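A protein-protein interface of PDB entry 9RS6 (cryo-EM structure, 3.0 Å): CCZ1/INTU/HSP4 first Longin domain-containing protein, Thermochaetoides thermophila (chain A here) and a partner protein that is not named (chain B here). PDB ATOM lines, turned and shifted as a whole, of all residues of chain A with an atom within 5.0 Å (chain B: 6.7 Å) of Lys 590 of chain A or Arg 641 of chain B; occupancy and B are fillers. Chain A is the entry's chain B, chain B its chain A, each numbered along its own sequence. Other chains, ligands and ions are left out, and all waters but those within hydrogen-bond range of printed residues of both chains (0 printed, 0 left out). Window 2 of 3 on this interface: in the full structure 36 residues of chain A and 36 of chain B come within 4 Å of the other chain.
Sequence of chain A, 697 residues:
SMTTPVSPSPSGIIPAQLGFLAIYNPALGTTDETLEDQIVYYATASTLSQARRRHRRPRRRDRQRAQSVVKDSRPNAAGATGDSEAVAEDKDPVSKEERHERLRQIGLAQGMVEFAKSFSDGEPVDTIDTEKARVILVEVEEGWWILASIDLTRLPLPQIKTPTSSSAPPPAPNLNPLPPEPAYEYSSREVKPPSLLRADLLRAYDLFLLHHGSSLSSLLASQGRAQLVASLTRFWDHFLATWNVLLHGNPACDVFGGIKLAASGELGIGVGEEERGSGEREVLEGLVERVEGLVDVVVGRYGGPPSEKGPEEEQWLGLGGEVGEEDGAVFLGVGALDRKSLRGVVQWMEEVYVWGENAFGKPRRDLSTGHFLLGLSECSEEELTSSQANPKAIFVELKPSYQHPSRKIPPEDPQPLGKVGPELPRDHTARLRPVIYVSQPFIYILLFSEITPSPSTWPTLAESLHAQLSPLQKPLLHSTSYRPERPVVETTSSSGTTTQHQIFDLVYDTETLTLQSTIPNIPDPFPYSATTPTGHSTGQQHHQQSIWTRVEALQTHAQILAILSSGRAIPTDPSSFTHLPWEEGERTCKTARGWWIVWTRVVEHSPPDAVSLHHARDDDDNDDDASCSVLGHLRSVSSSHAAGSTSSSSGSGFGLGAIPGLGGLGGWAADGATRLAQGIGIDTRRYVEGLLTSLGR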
ATOM      1  N   THR A 588       3.698   9.974 -18.273  1.00  0.00           N
ATOM      2  CA  THR A 588       5.120  10.003 -18.585  1.00  0.00           C
ATOM      3  C   THR A 588       5.470   8.889 -19.564  1.00  0.00           C
ATOM      4  O   THR A 588       5.046   7.741 -19.405  1.00  0.00           O
ATOM      5  CB  THR A 588       5.944   9.861 -17.306  1.00  0.00           C
ATOM      6  OG1 THR A 588       5.509  10.835 -16.349  1.00  0.00           O
ATOM      7  CG2 THR A 588       7.422  10.075 -17.593  1.00  0.00           C
ATOM      8  N   CYS A 589       6.252   9.232 -20.585  1.00  0.00           N
ATOM      9  CA  CYS A 589       6.619   8.288 -21.638  1.00  0.00           C
ATOM     10  C   CYS A 589       8.100   8.452 -21.955  1.00  0.00           C
ATOM     11  O   CYS A 589       8.564   9.564 -22.219  1.00  0.00           O
ATOM     12  CB  CYS A 589       5.766   8.502 -22.889  1.00  0.00           C
ATOM     13  SG  CYS A 589       3.989   8.279 -22.630  1.00  0.00           S
ATOM     14  N   LYS A 590       8.837   7.348 -21.936  1.00  0.00           N
ATOM     15  CA  LYS A 590      10.250   7.375 -22.280  1.00  0.00           C
ATOM     16  C   LYS A 590      10.444   6.860 -23.703  1.00  0.00           C
ATOM     17  O   LYS A 590       9.507   6.402 -24.360  1.00  0.00           O
ATOM     18  CB  LYS A 590      11.069   6.541 -21.292  1.00  0.00           C
ATOM     19  CG  LYS A 590      11.287   7.183 -19.921  1.00  0.00           C
ATOM     20  CD  LYS A 590      10.069   7.007 -19.018  1.00  0.00           C
ATOM     21  CE  LYS A 590      10.328   7.479 -17.600  1.00  0.00           C
ATOM     22  NZ  LYS A 590       9.126   7.322 -16.737  1.00  0.00           N
ATOM     23  N   THR A 591      11.682   6.946 -24.187  1.00  0.00           N
ATOM     24  CA  THR A 591      12.007   6.525 -25.543  1.00  0.00           C
ATOM     25  C   THR A 591      13.293   5.714 -25.532  1.00  0.00           C
ATOM     26  O   THR A 591      13.973   5.591 -24.510  1.00  0.00           O
ATOM     27  CB  THR A 591      12.180   7.715 -26.497  1.00  0.00           C
ATOM     28  OG1 THR A 591      13.256   8.540 -26.037  1.00  0.00           O
ATOM     29  CG2 THR A 591      10.914   8.539 -26.576  1.00  0.00           C
ATOM     30  N   ALA A 592      13.621   5.153 -26.698  1.00  0.00           N
ATOM     31  CA  ALA A 592      14.919   4.523 -26.892  1.00  0.00           C
ATOM     32  C   ALA A 592      15.997   5.527 -27.276  1.00  0.00           C
ATOM     33  O   ALA A 592      17.185   5.194 -27.213  1.00  0.00           O
ATOM     34  CB  ALA A 592      14.824   3.436 -27.964  1.00  0.00           C
ATOM     35  N   TRP A 595      14.377  10.535 -25.133  1.00  0.00           N
ATOM     36  CA  TRP A 595      13.374  11.592 -25.041  1.00  0.00           C
ATOM     37  C   TRP A 595      12.407  11.239 -23.916  1.00  0.00           C
ATOM     38  O   TRP A 595      11.832  10.146 -23.900  1.00  0.00           O
ATOM     39  CB  TRP A 595      12.649  11.760 -26.373  1.00  0.00           C
ATOM     40  CG  TRP A 595      11.859  13.020 -26.460  1.00  0.00           C
ATOM     41  CD1 TRP A 595      10.529  13.165 -26.226  1.00  0.00           C
ATOM     42  CD2 TRP A 595      12.351  14.320 -26.799  1.00  0.00           C
ATOM     43  NE1 TRP A 595      10.154  14.474 -26.400  1.00  0.00           N
ATOM     44  CE2 TRP A 595      11.258  15.204 -26.751  1.00  0.00           C
ATOM     45  CE3 TRP A 595      13.610  14.821 -27.137  1.00  0.00           C
ATOM     46  CZ2 TRP A 595      11.384  16.559 -27.033  1.00  0.00           C
ATOM     47  CZ3 TRP A 595      13.731  16.165 -27.418  1.00  0.00           C
ATOM     48  CH2 TRP A 595      12.628  17.020 -27.357  1.00  0.00           C
ATOM     49  N   TRP A 596      12.233  12.161 -22.972  1.00  0.00           N
ATOM     50  CA  TRP A 596      11.487  11.909 -21.737  1.00  0.00           C
ATOM     51  C   TRP A 596      10.294  12.859 -21.696  1.00  0.00           C
ATOM     52  O   TRP A 596      10.415  14.003 -21.266  1.00  0.00           O
ATOM     53  CB  TRP A 596      12.394  12.116 -20.528  1.00  0.00           C
ATOM     54  CG  TRP A 596      13.528  11.137 -20.411  1.00  0.00           C
ATOM     55  CD1 TRP A 596      14.612  11.043 -21.232  1.00  0.00           C
ATOM     56  CD2 TRP A 596      13.736  10.180 -19.364  1.00  0.00           C
ATOM     57  NE1 TRP A 596      15.457  10.054 -20.794  1.00  0.00           N
ATOM     58  CE2 TRP A 596      14.944   9.512 -19.644  1.00  0.00           C
ATOM     59  CE3 TRP A 596      13.009   9.810 -18.229  1.00  0.00           C
ATOM     60  CZ2 TRP A 596      15.441   8.495 -18.831  1.00  0.00           C
ATOM     61  CZ3 TRP A 596      13.507   8.800 -17.422  1.00  0.00           C
ATOM     62  CH2 TRP A 596      14.709   8.152 -17.729  1.00  0.00           C
ATOM     63  N   LEU B 597       2.682   1.522 -25.492  1.00  0.00           N
ATOM     64  CA  LEU B 597       3.978   0.994 -25.907  1.00  0.00           C
ATOM     65  C   LEU B 597       3.960   0.561 -27.369  1.00  0.00           C
ATOM     66  O   LEU B 597       4.831   0.951 -28.155  1.00  0.00           O
ATOM     67  CB  LEU B 597       4.398  -0.183 -25.021  1.00  0.00           C
ATOM     68  CG  LEU B 597       5.097   0.068 -23.679  1.00  0.00           C
ATOM     69  CD1 LEU B 597       6.349   0.915 -23.868  1.00  0.00           C
ATOM     70  CD2 LEU B 597       4.188   0.656 -22.622  1.00  0.00           C
ATOM     71  N   HIS B 603       8.259   5.039 -31.089  1.00  0.00           N
ATOM     72  CA  HIS B 603       9.228   4.159 -30.432  1.00  0.00           C
ATOM     73  C   HIS B 603       9.335   4.518 -28.949  1.00  0.00           C
ATOM     74  O   HIS B 603      10.267   5.183 -28.492  1.00  0.00           O
ATOM     75  CB  HIS B 603      10.580   4.245 -31.129  1.00  0.00           C
ATOM     76  CG  HIS B 603      10.571   3.725 -32.533  1.00  0.00           C
ATOM     77  ND1 HIS B 603      10.264   4.520 -33.617  1.00  0.00           N
ATOM     78  CD2 HIS B 603      10.833   2.494 -33.033  1.00  0.00           C
ATOM     79  CE1 HIS B 603      10.336   3.801 -34.723  1.00  0.00           C
ATOM     80  NE2 HIS B 603      10.680   2.567 -34.395  1.00  0.00           N
ATOM     81  N   LEU B 604       8.345   4.052 -28.190  1.00  0.00           N
ATOM     82  CA  LEU B 604       8.280   4.305 -26.753  1.00  0.00           C
ATOM     83  C   LEU B 604       8.845   3.101 -26.009  1.00  0.00           C
ATOM     84  O   LEU B 604       8.426   1.962 -26.241  1.00  0.00           O
ATOM     85  CB  LEU B 604       6.850   4.612 -26.315  1.00  0.00           C
ATOM     86  CG  LEU B 604       6.337   6.039 -26.551  1.00  0.00           C
ATOM     87  CD1 LEU B 604       6.080   6.336 -28.011  1.00  0.00           C
ATOM     88  CD2 LEU B 604       5.080   6.297 -25.746  1.00  0.00           C
ATOM     89  N   ARG B 605       9.807   3.356 -25.121  1.00  0.00           N
ATOM     90  CA  ARG B 605      10.443   2.275 -24.377  1.00  0.00           C
ATOM     91  C   ARG B 605       9.757   2.052 -23.035  1.00  0.00           C
ATOM     92  O   ARG B 605       9.425   0.917 -22.676  1.00  0.00           O
ATOM     93  CB  ARG B 605      11.928   2.582 -24.186  1.00  0.00           C
ATOM     94  CG  ARG B 605      12.737   1.441 -23.599  1.00  0.00           C
ATOM     95  CD  ARG B 605      12.499   0.149 -24.358  1.00  0.00           C
ATOM     96  NE  ARG B 605      12.755   0.278 -25.789  1.00  0.00           N
ATOM     97  CZ  ARG B 605      13.932   0.061 -26.360  1.00  0.00           C
ATOM     98  NH1 ARG B 605      14.996  -0.269 -25.647  1.00  0.00           N
ATOM     99  NH2 ARG B 605      14.043   0.174 -27.681  1.00  0.00           N
ATOM    100  N   VAL B 606       9.544   3.125 -22.277  1.00  0.00           N
ATOM    101  CA  VAL B 606       8.899   3.064 -20.971  1.00  0.00           C
ATOM    102  C   VAL B 606       7.754   4.065 -20.955  1.00  0.00           C
ATOM    103  O   VAL B 606       7.923   5.219 -21.363  1.00  0.00           O
ATOM    104  CB  VAL B 606       9.893   3.362 -19.827  1.00  0.00           C
ATOM    105  CG1 VAL B 606       9.175   3.417 -18.490  1.00  0.00           C
ATOM    106  CG2 VAL B 606      10.999   2.326 -19.796  1.00  0.00           C
ATOM    107  N   VAL B 607       6.588   3.623 -20.494  1.00  0.00           N
ATOM    108  CA  VAL B 607       5.411   4.478 -20.384  1.00  0.00           C
ATOM    109  C   VAL B 607       4.901   4.417 -18.952  1.00  0.00           C
ATOM    110  O   VAL B 607       4.714   3.329 -18.403  1.00  0.00           O
ATOM    111  CB  VAL B 607       4.303   4.058 -21.367  1.00  0.00           C
ATOM    112  CG1 VAL B 607       3.031   4.850 -21.113  1.00  0.00           C
ATOM    113  CG2 VAL B 607       4.770   4.249 -22.791  1.00  0.00           C
ATOM    114  N   TYR B 608       4.671   5.581 -18.354  1.00  0.00           N
ATOM    115  CA  TYR B 608       4.150   5.667 -16.999  1.00  0.00           C
ATOM    116  C   TYR B 608       2.875   6.495 -17.008  1.00  0.00           C
ATOM    117  O   TYR B 608       2.752   7.463 -17.762  1.00  0.00           O
ATOM    118  CB  TYR B 608       5.185   6.282 -16.047  1.00  0.00           C
ATOM    119  CG  TYR B 608       4.655   6.619 -14.673  1.00  0.00           C
ATOM    120  CD1 TYR B 608       4.457   5.626 -13.725  1.00  0.00           C
ATOM    121  CD2 TYR B 608       4.365   7.929 -14.321  1.00  0.00           C
ATOM    122  CE1 TYR B 608       3.979   5.927 -12.466  1.00  0.00           C
ATOM    123  CE2 TYR B 608       3.885   8.239 -13.064  1.00  0.00           C
ATOM    124  CZ  TYR B 608       3.695   7.235 -12.141  1.00  0.00           C
ATOM    125  OH  TYR B 608       3.217   7.539 -10.888  1.00  0.00           O
ATOM    126  N   LEU B 622       3.215   1.308 -14.908  1.00  0.00           N
ATOM    127  CA  LEU B 622       4.375   1.443 -15.776  1.00  0.00           C
ATOM    128  C   LEU B 622       4.455   0.244 -16.708  1.00  0.00           C
ATOM    129  O   LEU B 622       4.136  -0.886 -16.321  1.00  0.00           O
ATOM    130  CB  LEU B 622       5.676   1.572 -14.968  1.00  0.00           C
ATOM    131  CG  LEU B 622       6.962   1.993 -15.687  1.00  0.00           C
ATOM    132  CD1 LEU B 622       7.828   2.823 -14.756  1.00  0.00           C
ATOM    133  CD2 LEU B 622       7.751   0.797 -16.201  1.00  0.00           C
ATOM    134  N   VAL B 639       3.108   6.699  -5.127  1.00  0.00           N
ATOM    135  CA  VAL B 639       4.422   6.073  -5.249  1.00  0.00           C
ATOM    136  C   VAL B 639       5.423   7.021  -5.902  1.00  0.00           C
ATOM    137  O   VAL B 639       6.564   7.143  -5.442  1.00  0.00           O
ATOM    138  CB  VAL B 639       4.339   4.737  -6.013  1.00  0.00           C
ATOM    139  CG1 VAL B 639       3.696   3.672  -5.141  1.00  0.00           C
ATOM    140  CG2 VAL B 639       3.560   4.893  -7.309  1.00  0.00           C
ATOM    141  N   GLY B 640       5.014   7.699  -6.971  1.00  0.00           N
ATOM    142  CA  GLY B 640       5.924   8.497  -7.764  1.00  0.00           C
ATOM    143  C   GLY B 640       6.589   7.683  -8.859  1.00  0.00           C
ATOM    144  O   GLY B 640       6.529   6.454  -8.897  1.00  0.00           O
ATOM    145  N   ARG B 641       7.244   8.400  -9.777  1.00  0.00           N
ATOM    146  CA  ARG B 641       7.855   7.751 -10.934  1.00  0.00           C
ATOM    147  C   ARG B 641       8.991   6.825 -10.514  1.00  0.00           C
ATOM    148  O   ARG B 641       8.976   5.627 -10.819  1.00  0.00           O
ATOM    149  CB  ARG B 641       8.350   8.817 -11.918  1.00  0.00           C
ATOM    150  CG  ARG B 641       8.719   8.319 -13.322  1.00  0.00           C
ATOM    151  CD  ARG B 641      10.168   7.841 -13.430  1.00  0.00           C
ATOM    152  NE  ARG B 641      11.087   8.655 -12.640  1.00  0.00           N
ATOM    153  CZ  ARG B 641      11.526   9.856 -12.992  1.00  0.00           C
ATOM    154  NH1 ARG B 641      11.163  10.420 -14.133  1.00  0.00           N
ATOM    155  NH2 ARG B 641      12.353  10.508 -12.180  1.00  0.00           N
ATOM    156  N   ALA B 642       9.984   7.366  -9.806  1.00  0.00           N
ATOM    157  CA  ALA B 642      11.156   6.574  -9.444  1.00  0.00           C
ATOM    158  C   ALA B 642      10.815   5.517  -8.402  1.00  0.00           C
ATOM    159  O   ALA B 642      11.353   4.402  -8.443  1.00  0.00           O
ATOM    160  CB  ALA B 642      12.270   7.488  -8.937  1.00  0.00           C
ATOM    161  N   GLY B 643       9.911   5.842  -7.475  1.00  0.00           N
ATOM    162  CA  GLY B 643       9.574   4.939  -6.387  1.00  0.00           C
ATOM    163  C   GLY B 643       8.944   3.635  -6.829  1.00  0.00           C
ATOM    164  O   GLY B 643       8.899   2.686  -6.040  1.00  0.00           O
ATOM    165  N   MET B 644       8.458   3.565  -8.064  1.00  0.00           N
ATOM    166  CA  MET B 644       7.927   2.328  -8.617  1.00  0.00           C
ATOM    167  C   MET B 644       8.658   1.877  -9.872  1.00  0.00           C
ATOM    168  O   MET B 644       8.570   0.706 -10.246  1.00  0.00           O
ATOM    169  CB  MET B 644       6.421   2.479  -8.878  1.00  0.00           C
ATOM    170  CG  MET B 644       6.017   3.551  -9.871  1.00  0.00           C
ATOM    171  SD  MET B 644       6.050   3.032 -11.586  1.00  0.00           S
ATOM    172  CE  MET B 644       4.611   1.972 -11.565  1.00  0.00           C
ATOM    173  N   ALA B 645       9.427   2.762 -10.513  1.00  0.00           N
ATOM    174  CA  ALA B 645      10.405   2.301 -11.492  1.00  0.00           C
ATOM    175  C   ALA B 645      11.483   1.446 -10.838  1.00  0.00           C
ATOM    176  O   ALA B 645      11.983   0.502 -11.464  1.00  0.00           O
ATOM    177  CB  ALA B 645      11.038   3.490 -12.211  1.00  0.00           C
ATOM    178  N   ARG B 646      11.841   1.752  -9.589  1.00  0.00           N
ATOM    179  CA  ARG B 646      12.708   0.864  -8.824  1.00  0.00           C
ATOM    180  C   ARG B 646      12.074  -0.512  -8.661  1.00  0.00           C
ATOM    181  O   ARG B 646      12.757  -1.538  -8.769  1.00  0.00           O
ATOM    182  CB  ARG B 646      13.002   1.484  -7.459  1.00  0.00           C
ATOM    183  CG  ARG B 646      13.884   0.648  -6.553  1.00  0.00           C
ATOM    184  CD  ARG B 646      14.076   1.347  -5.222  1.00  0.00           C
ATOM    185  NE  ARG B 646      12.807   1.509  -4.522  1.00  0.00           N
ATOM    186  CZ  ARG B 646      12.633   2.269  -3.450  1.00  0.00           C
ATOM    187  NH1 ARG B 646      13.630   2.956  -2.920  1.00  0.00           N
ATOM    188  NH2 ARG B 646      11.424   2.344  -2.898  1.00  0.00           N
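N of Arg 605 of chain B is in hydrogen-bond range of O of Lys 590 of chain A, 3.2 Å away.
The backbone carbonyl oxygen (O) of Val 606 of chain B sits close to the backbone NH (N) of Lys 590 of chain A.
The backbone carbonyl oxygen (O) of Thr 588 of chain A is in hydrogen-bond range of the backbone NH (N) of Tyr 608 of chain B, at 2.4 Å.
The side-chain hydroxyl (OG1) of Thr 591 of chain A sits at hydrogen-bond distance from the backbone NH (N) of Trp 595 of chain A (2.5 Å).
Among the printed residues, pairs that only touch across the chains: Thr 588 of chain A with Val 607 of chain B (3.4 Å), Cys 589 of chain A with Leu 604 of chain B (3.7 Å), Cys 589 of chain A with Val 606 of chain B (3.3 Å), Cys 589 of chain A with Val 607 of chain B (3.9 Å), Lys 590 of chain A with Leu 604 of chain B (3.4 Å), Lys 590 of chain A with Arg 641 of chain B (3.5 Å), Thr 591 of chain A with His 603 of chain B (3.7 Å), Thr 591 of chain A with Arg 605 of chain B (3.7 Å), Ala 592 of chain A with His 603 of chain B (3.8 Å) and Ala 592 of chain A with Arg 605 of chain B (3.4 Å).
Of the printed residues of chain B, Thr 591 of chain A touches His 603 and Arg 605.
Of the printed residues of chain A, His 603 of chain B touches Thr 591 and Ala 592.
Arg 646 of chain B touches none of the printed residues of chain A.
The nearest residue of chain B that does not touch Lys 590 of chain A is Tyr 608 of chain B (4.1 Å).
The nearest printed residue of chain A that does not touch Tyr 608 of chain B is Lys 590 of chain A (4.1 Å).
Of the 16 printed residues of chain B, 7 touch a printed residue of chain A.
Hydrophobic or aromatic side chains of chain B within 4 Å of the printed part of chain A: Leu 604, Val 606, Val 607 and Tyr 608.
Among the printed residues, 13 pairs touch across the chains.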
